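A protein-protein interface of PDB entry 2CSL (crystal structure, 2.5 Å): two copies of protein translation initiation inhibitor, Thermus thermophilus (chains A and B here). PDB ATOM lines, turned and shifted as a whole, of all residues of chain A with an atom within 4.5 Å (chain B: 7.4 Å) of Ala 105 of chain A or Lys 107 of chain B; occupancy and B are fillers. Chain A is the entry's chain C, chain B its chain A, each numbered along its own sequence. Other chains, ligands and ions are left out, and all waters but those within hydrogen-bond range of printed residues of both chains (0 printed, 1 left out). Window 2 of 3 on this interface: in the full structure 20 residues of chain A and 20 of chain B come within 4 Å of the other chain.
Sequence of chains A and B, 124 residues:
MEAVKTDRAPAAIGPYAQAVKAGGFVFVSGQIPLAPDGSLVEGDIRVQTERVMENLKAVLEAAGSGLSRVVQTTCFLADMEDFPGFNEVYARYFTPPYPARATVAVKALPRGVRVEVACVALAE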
ATOM      1  N   LEU A  77     -22.150 -25.869  18.449  1.00  0.00           N
ATOM      2  CA  LEU A  77     -23.462 -26.296  17.957  1.00  0.00           C
ATOM      3  C   LEU A  77     -24.547 -25.563  18.746  1.00  0.00           C
ATOM      4  O   LEU A  77     -24.333 -25.200  19.905  1.00  0.00           O
ATOM      5  CB  LEU A  77     -23.646 -27.805  18.147  1.00  0.00           C
ATOM      6  CG  LEU A  77     -22.698 -28.760  17.419  1.00  0.00           C
ATOM      7  CD1 LEU A  77     -22.907 -30.176  17.930  1.00  0.00           C
ATOM      8  CD2 LEU A  77     -22.936 -28.677  15.921  1.00  0.00           C
ATOM      9  N   ALA A  78     -25.707 -25.346  18.127  1.00  0.00           N
ATOM     10  CA  ALA A  78     -26.811 -24.666  18.803  1.00  0.00           C
ATOM     11  C   ALA A  78     -27.623 -25.670  19.618  1.00  0.00           C
ATOM     12  O   ALA A  78     -28.511 -25.288  20.383  1.00  0.00           O
ATOM     13  CB  ALA A  78     -27.719 -23.968  17.778  1.00  0.00           C
ATOM     14  N   MET A  80     -26.896 -29.860  21.235  1.00  0.00           N
ATOM     15  CA  MET A  80     -26.137 -31.110  21.292  1.00  0.00           C
ATOM     16  C   MET A  80     -26.830 -32.308  20.626  1.00  0.00           C
ATOM     17  O   MET A  80     -26.167 -33.253  20.206  1.00  0.00           O
ATOM     18  CB  MET A  80     -25.808 -31.437  22.751  1.00  0.00           C
ATOM     19  CG  MET A  80     -24.469 -32.149  22.980  1.00  0.00           C
ATOM     20  SD  MET A  80     -22.851 -31.119  22.556  1.00  0.00           S
ATOM     21  CE  MET A  80     -22.077 -32.327  21.282  1.00  0.00           C
ATOM     22  N   VAL A 104     -18.900 -28.077  21.654  1.00  0.00           N
ATOM     23  CA  VAL A 104     -19.775 -27.521  22.677  1.00  0.00           C
ATOM     24  C   VAL A 104     -21.101 -27.020  22.090  1.00  0.00           C
ATOM     25  O   VAL A 104     -21.204 -26.709  20.896  1.00  0.00           O
ATOM     26  CB  VAL A 104     -19.079 -26.325  23.398  1.00  0.00           C
ATOM     27  CG1 VAL A 104     -20.048 -25.632  24.314  1.00  0.00           C
ATOM     28  CG2 VAL A 104     -17.885 -26.803  24.200  1.00  0.00           C
ATOM     29  N   ALA A 105     -22.115 -26.952  22.947  1.00  0.00           N
ATOM     30  CA  ALA A 105     -23.428 -26.450  22.569  1.00  0.00           C
ATOM     31  C   ALA A 105     -23.490 -25.055  23.183  1.00  0.00           C
ATOM     32  O   ALA A 105     -23.260 -24.884  24.380  1.00  0.00           O
ATOM     33  CB  ALA A 105     -24.520 -27.331  23.156  1.00  0.00           C
ATOM     34  N   VAL A 106     -23.779 -24.051  22.369  1.00  0.00           N
ATOM     35  CA  VAL A 106     -23.849 -22.690  22.879  1.00  0.00           C
ATOM     36  C   VAL A 106     -25.266 -22.151  22.819  1.00  0.00           C
ATOM     37  O   VAL A 106     -26.144 -22.763  22.220  1.00  0.00           O
ATOM     38  CB  VAL A 106     -22.918 -21.757  22.090  1.00  0.00           C
ATOM     39  CG1 VAL A 106     -21.479 -22.132  22.361  1.00  0.00           C
ATOM     40  CG2 VAL A 106     -23.217 -21.855  20.598  1.00  0.00           C
ATOM     41  N   LYS A 107     -25.476 -20.997  23.444  1.00  0.00           N
ATOM     42  CA  LYS A 107     -26.784 -20.359  23.485  1.00  0.00           C
ATOM     43  C   LYS A 107     -27.292 -19.995  22.093  1.00  0.00           C
ATOM     44  O   LYS A 107     -28.422 -20.315  21.740  1.00  0.00           O
ATOM     45  CB  LYS A 107     -26.710 -19.105  24.363  1.00  0.00           C
ATOM     46  CG  LYS A 107     -28.054 -18.453  24.650  1.00  0.00           C
ATOM     47  CD  LYS A 107     -27.905 -17.287  25.619  1.00  0.00           C
ATOM     48  CE  LYS A 107     -29.252 -16.674  25.975  1.00  0.00           C
ATOM     49  NZ  LYS A 107     -29.089 -15.557  26.942  1.00  0.00           N
ATOM     50  N   PHE B  76     -14.731 -24.864  29.487  1.00  0.00           N
ATOM     51  CA  PHE B  76     -16.178 -24.755  29.333  1.00  0.00           C
ATOM     52  C   PHE B  76     -16.905 -25.411  30.512  1.00  0.00           C
ATOM     53  O   PHE B  76     -16.695 -26.592  30.802  1.00  0.00           O
ATOM     54  CB  PHE B  76     -16.632 -25.425  28.026  1.00  0.00           C
ATOM     55  CG  PHE B  76     -15.911 -24.937  26.792  1.00  0.00           C
ATOM     56  CD1 PHE B  76     -14.711 -25.521  26.388  1.00  0.00           C
ATOM     57  CD2 PHE B  76     -16.453 -23.921  26.009  1.00  0.00           C
ATOM     58  CE1 PHE B  76     -14.066 -25.103  25.218  1.00  0.00           C
ATOM     59  CE2 PHE B  76     -15.820 -23.496  24.839  1.00  0.00           C
ATOM     60  CZ  PHE B  76     -14.626 -24.089  24.441  1.00  0.00           C
ATOM     61  N   LEU B  77     -17.754 -24.643  31.190  1.00  0.00           N
ATOM     62  CA  LEU B  77     -18.523 -25.162  32.321  1.00  0.00           C
ATOM     63  C   LEU B  77     -19.999 -25.156  31.937  1.00  0.00           C
ATOM     64  O   LEU B  77     -20.432 -24.338  31.124  1.00  0.00           O
ATOM     65  CB  LEU B  77     -18.325 -24.293  33.564  1.00  0.00           C
ATOM     66  CG  LEU B  77     -16.905 -24.079  34.105  1.00  0.00           C
ATOM     67  CD1 LEU B  77     -16.962 -23.091  35.261  1.00  0.00           C
ATOM     68  CD2 LEU B  77     -16.292 -25.403  34.561  1.00  0.00           C
ATOM     69  N   ALA B  78     -20.769 -26.070  32.520  1.00  0.00           N
ATOM     70  CA  ALA B  78     -22.197 -26.160  32.232  1.00  0.00           C
ATOM     71  C   ALA B  78     -22.967 -25.151  33.080  1.00  0.00           C
ATOM     72  O   ALA B  78     -24.012 -24.648  32.675  1.00  0.00           O
ATOM     73  CB  ALA B  78     -22.695 -27.577  32.511  1.00  0.00           C
ATOM     74  N   ASP B  79     -22.431 -24.858  34.258  1.00  0.00           N
ATOM     75  CA  ASP B  79     -23.042 -23.912  35.180  1.00  0.00           C
ATOM     76  C   ASP B  79     -21.903 -23.042  35.706  1.00  0.00           C
ATOM     77  O   ASP B  79     -20.874 -23.566  36.132  1.00  0.00           O
ATOM     78  CB  ASP B  79     -23.699 -24.676  36.335  1.00  0.00           C
ATOM     79  CG  ASP B  79     -24.466 -23.770  37.283  1.00  0.00           C
ATOM     80  OD1 ASP B  79     -23.983 -22.656  37.576  1.00  0.00           O
ATOM     81  OD2 ASP B  79     -25.552 -24.180  37.746  1.00  0.00           O
ATOM     82  N   ALA B 105     -19.406 -20.314  30.460  1.00  0.00           N
ATOM     83  CA  ALA B 105     -20.473 -21.278  30.723  1.00  0.00           C
ATOM     84  C   ALA B 105     -21.278 -21.436  29.432  1.00  0.00           C
ATOM     85  O   ALA B 105     -21.752 -20.449  28.863  1.00  0.00           O
ATOM     86  CB  ALA B 105     -21.377 -20.780  31.856  1.00  0.00           C
ATOM     87  N   VAL B 106     -21.420 -22.677  28.972  1.00  0.00           N
ATOM     88  CA  VAL B 106     -22.141 -22.977  27.740  1.00  0.00           C
ATOM     89  C   VAL B 106     -23.484 -23.645  28.007  1.00  0.00           C
ATOM     90  O   VAL B 106     -23.797 -23.952  29.155  1.00  0.00           O
ATOM     91  CB  VAL B 106     -21.301 -23.891  26.862  1.00  0.00           C
ATOM     92  CG1 VAL B 106     -20.004 -23.188  26.504  1.00  0.00           C
ATOM     93  CG2 VAL B 106     -21.008 -25.190  27.596  1.00  0.00           C
ATOM     94  N   LYS B 107     -24.274 -23.876  26.958  1.00  0.00           N
ATOM     95  CA  LYS B 107     -25.585 -24.506  27.134  1.00  0.00           C
ATOM     96  C   LYS B 107     -25.517 -25.980  27.531  1.00  0.00           C
ATOM     97  O   LYS B 107     -26.293 -26.442  28.366  1.00  0.00           O
ATOM     98  CB  LYS B 107     -26.446 -24.368  25.870  1.00  0.00           C
ATOM     99  CG  LYS B 107     -27.745 -25.167  25.966  1.00  0.00           C
ATOM    100  CD  LYS B 107     -28.910 -24.566  25.192  1.00  0.00           C
ATOM    101  CE  LYS B 107     -28.926 -24.983  23.734  1.00  0.00           C
ATOM    102  NZ  LYS B 107     -30.270 -24.725  23.125  1.00  0.00           N
ATOM    103  N   ALA B 108     -24.594 -26.719  26.931  1.00  0.00           N
ATOM    104  CA  ALA B 108     -24.446 -28.134  27.246  1.00  0.00           C
ATOM    105  C   ALA B 108     -23.125 -28.673  26.721  1.00  0.00           C
ATOM    106  O   ALA B 108     -22.552 -28.147  25.758  1.00  0.00           O
ATOM    107  CB  ALA B 108     -25.602 -28.928  26.653  1.00  0.00           C
ATOM    108  N   LEU B 109     -22.655 -29.736  27.360  1.00  0.00           N
ATOM    109  CA  LEU B 109     -21.396 -30.366  26.987  1.00  0.00           C
ATOM    110  C   LEU B 109     -21.623 -31.804  26.569  1.00  0.00           C
ATOM    111  O   LEU B 109     -22.682 -32.375  26.825  1.00  0.00           O
ATOM    112  CB  LEU B 109     -20.438 -30.340  28.169  1.00  0.00           C
ATOM    113  CG  LEU B 109     -19.952 -28.955  28.556  1.00  0.00           C
ATOM    114  CD1 LEU B 109     -19.203 -29.016  29.887  1.00  0.00           C
ATOM    115  CD2 LEU B 109     -19.073 -28.429  27.425  1.00  0.00           C
ATOM    116  N   PRO B 110     -20.628 -32.410  25.910  1.00  0.00           N
ATOM    117  CA  PRO B 110     -20.781 -33.802  25.483  1.00  0.00           C
ATOM    118  C   PRO B 110     -21.184 -34.679  26.665  1.00  0.00           C
ATOM    119  O   PRO B 110     -20.632 -34.556  27.759  1.00  0.00           O
ATOM    120  CB  PRO B 110     -19.395 -34.145  24.940  1.00  0.00           C
ATOM    121  CG  PRO B 110     -18.950 -32.837  24.351  1.00  0.00           C
ATOM    122  CD  PRO B 110     -19.353 -31.847  25.432  1.00  0.00           C
ATOM    123  N   VAL B 113     -22.021 -33.811  30.644  1.00  0.00           N
ATOM    124  CA  VAL B 113     -20.941 -33.501  31.567  1.00  0.00           C
ATOM    125  C   VAL B 113     -20.949 -32.030  32.002  1.00  0.00           C
ATOM    126  O   VAL B 113     -21.580 -31.187  31.353  1.00  0.00           O
ATOM    127  CB  VAL B 113     -19.614 -33.869  30.897  1.00  0.00           C
ATOM    128  CG1 VAL B 113     -18.557 -32.822  31.181  1.00  0.00           C
ATOM    129  CG2 VAL B 113     -19.197 -35.254  31.356  1.00  0.00           C
ATOM    130  N   GLU B 116     -15.366 -29.273  30.476  1.00  0.00           N
ATOM    131  CA  GLU B 116     -14.617 -29.663  29.293  1.00  0.00           C
ATOM    132  C   GLU B 116     -13.477 -28.675  29.195  1.00  0.00           C
ATOM    133  O   GLU B 116     -13.704 -27.467  29.178  1.00  0.00           O
ATOM    134  CB  GLU B 116     -15.449 -29.574  28.012  1.00  0.00           C
ATOM    135  CG  GLU B 116     -14.704 -30.169  26.798  1.00  0.00           C
ATOM    136  CD  GLU B 116     -15.465 -30.046  25.485  1.00  0.00           C
ATOM    137  OE1 GLU B 116     -16.705 -30.144  25.494  1.00  0.00           O
ATOM    138  OE2 GLU B 116     -14.815 -29.870  24.436  1.00  0.00           O
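Of the 12 printed residues of chain B, 6 touch a printed residue of chain A. Hydrophobic or aromatic side chains of chain B within 4 Å of the printed part of chain A: Phe 76, Val 106, Ala 108 and Leu 109. Of the 7 printed residues of chain A, 4 touch a printed residue of chain B. Printed residues of chain A that touch a printed residue of chain B: Ala 78, Val 104, Ala 105 and Val 106. Hydrophobic or aromatic side chains of chain A that line the printed part of chain B: Val 104 and Ala 105. Among the printed residues, 10 pairs touch across the chains. Among the printed residues, no Asp or Glu carboxylate lies within 4 Å of a Lys or Arg side-chain nitrogen of the other chain.
The backbone carbonyl oxygen (O) of Ala 105 of chain A sits at hydrogen-bond distance from the backbone NH (N) of Lys 107 of chain B (2.9 Å). The side-chain amino group (NZ) of Lys 107 of chain B is in hydrogen-bond range of the backbone carbonyl oxygen (O) of Ala 78 of chain A (3.3 Å). The backbone NH of Ala 105 of chain A lies within hydrogen-bond range of the backbone carbonyl oxygen of Ala 108 of chain B, 3.1 Å away.
The backbone carbonyl oxygen (O) of Leu 77 of chain B is in hydrogen-bond range of the backbone NH (N) of Val 106 of chain B. N of Phe 76 of chain B lies within hydrogen-bond range of O of Glu 116 of chain B (2.8 Å). N of Leu 77 of chain A is in hydrogen-bond range of O of Val 104 of chain A (2.8 Å). The backbone carbonyl oxygen (O) of Leu 77 of chain A lies within hydrogen-bond range of the backbone NH (N) of Val 106 of chain A.
Val 104 of chain A touches Phe 76 of chain B (CG2 to CD2, 3.7 Å). Val 104 of chain A touches Val 106 of chain B (CG1 to CG1, 3.3 Å). Val 104 of chain A touches Ala 108 of chain B (CG1 to O, 3.8 Å). CD2 of Leu 109 of chain B touches CG2 of Val 104 of chain A (3.8 Å). Val 104 of chain A touches Glu 116 of chain B (CG2 to OE1, 3.8 Å). Val 106 of chain B touches Ala 105 of chain A. Lys 107 of chain B touches Val 106 of chain A (CE to O, 3.9 Å).
Of chain A, only Ala 78, Ala 105 and Val 106 come within 4 Å of Lys 107 of chain B. Of the printed residues of chain B, Val 106 of chain A touches Lys 107. Of the printed residues of chain B, Val 104 of chain A touches Phe 76, Val 106, Ala 108, Leu 109 and Glu 116. Val 113 of chain B touches none of the printed residues of chain A. The nearest residue of chain B that does not touch Ala 105 of chain A is Leu 109 of chain B (5.2 Å). The nearest residue of chain A that does not touch Lys 107 of chain B is Lys 107 of chain A (4.3 Å). The nearest printed residue of chain B that does not touch Val 104 of chain A is Pro 110 of chain B (5.1 Å).
Ala 78 of chain A touches Lys 107 of chain B, but with the chains exchanged Lys 107 of chain A does not touch Ala 78 of chain B (10.0 Å). Ala 105 of chain A touches Val 106 of chain B, but with the chains exchanged Val 106 of chain A does not touch Ala 105 of chain B (6.7 Å). Ala 105 of chain A touches Lys 107 of chain B, but with the chains exchanged Lys 107 of chain A does not touch Ala 105 of chain B (6.6 Å). Val 106 of chain A touches Lys 107 of chain B, but with the chains exchanged Lys 107 of chain A does not touch Val 106 of chain B (5.6 Å). Positions printed for both chains: 77, 78, 105, 106 and 107.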
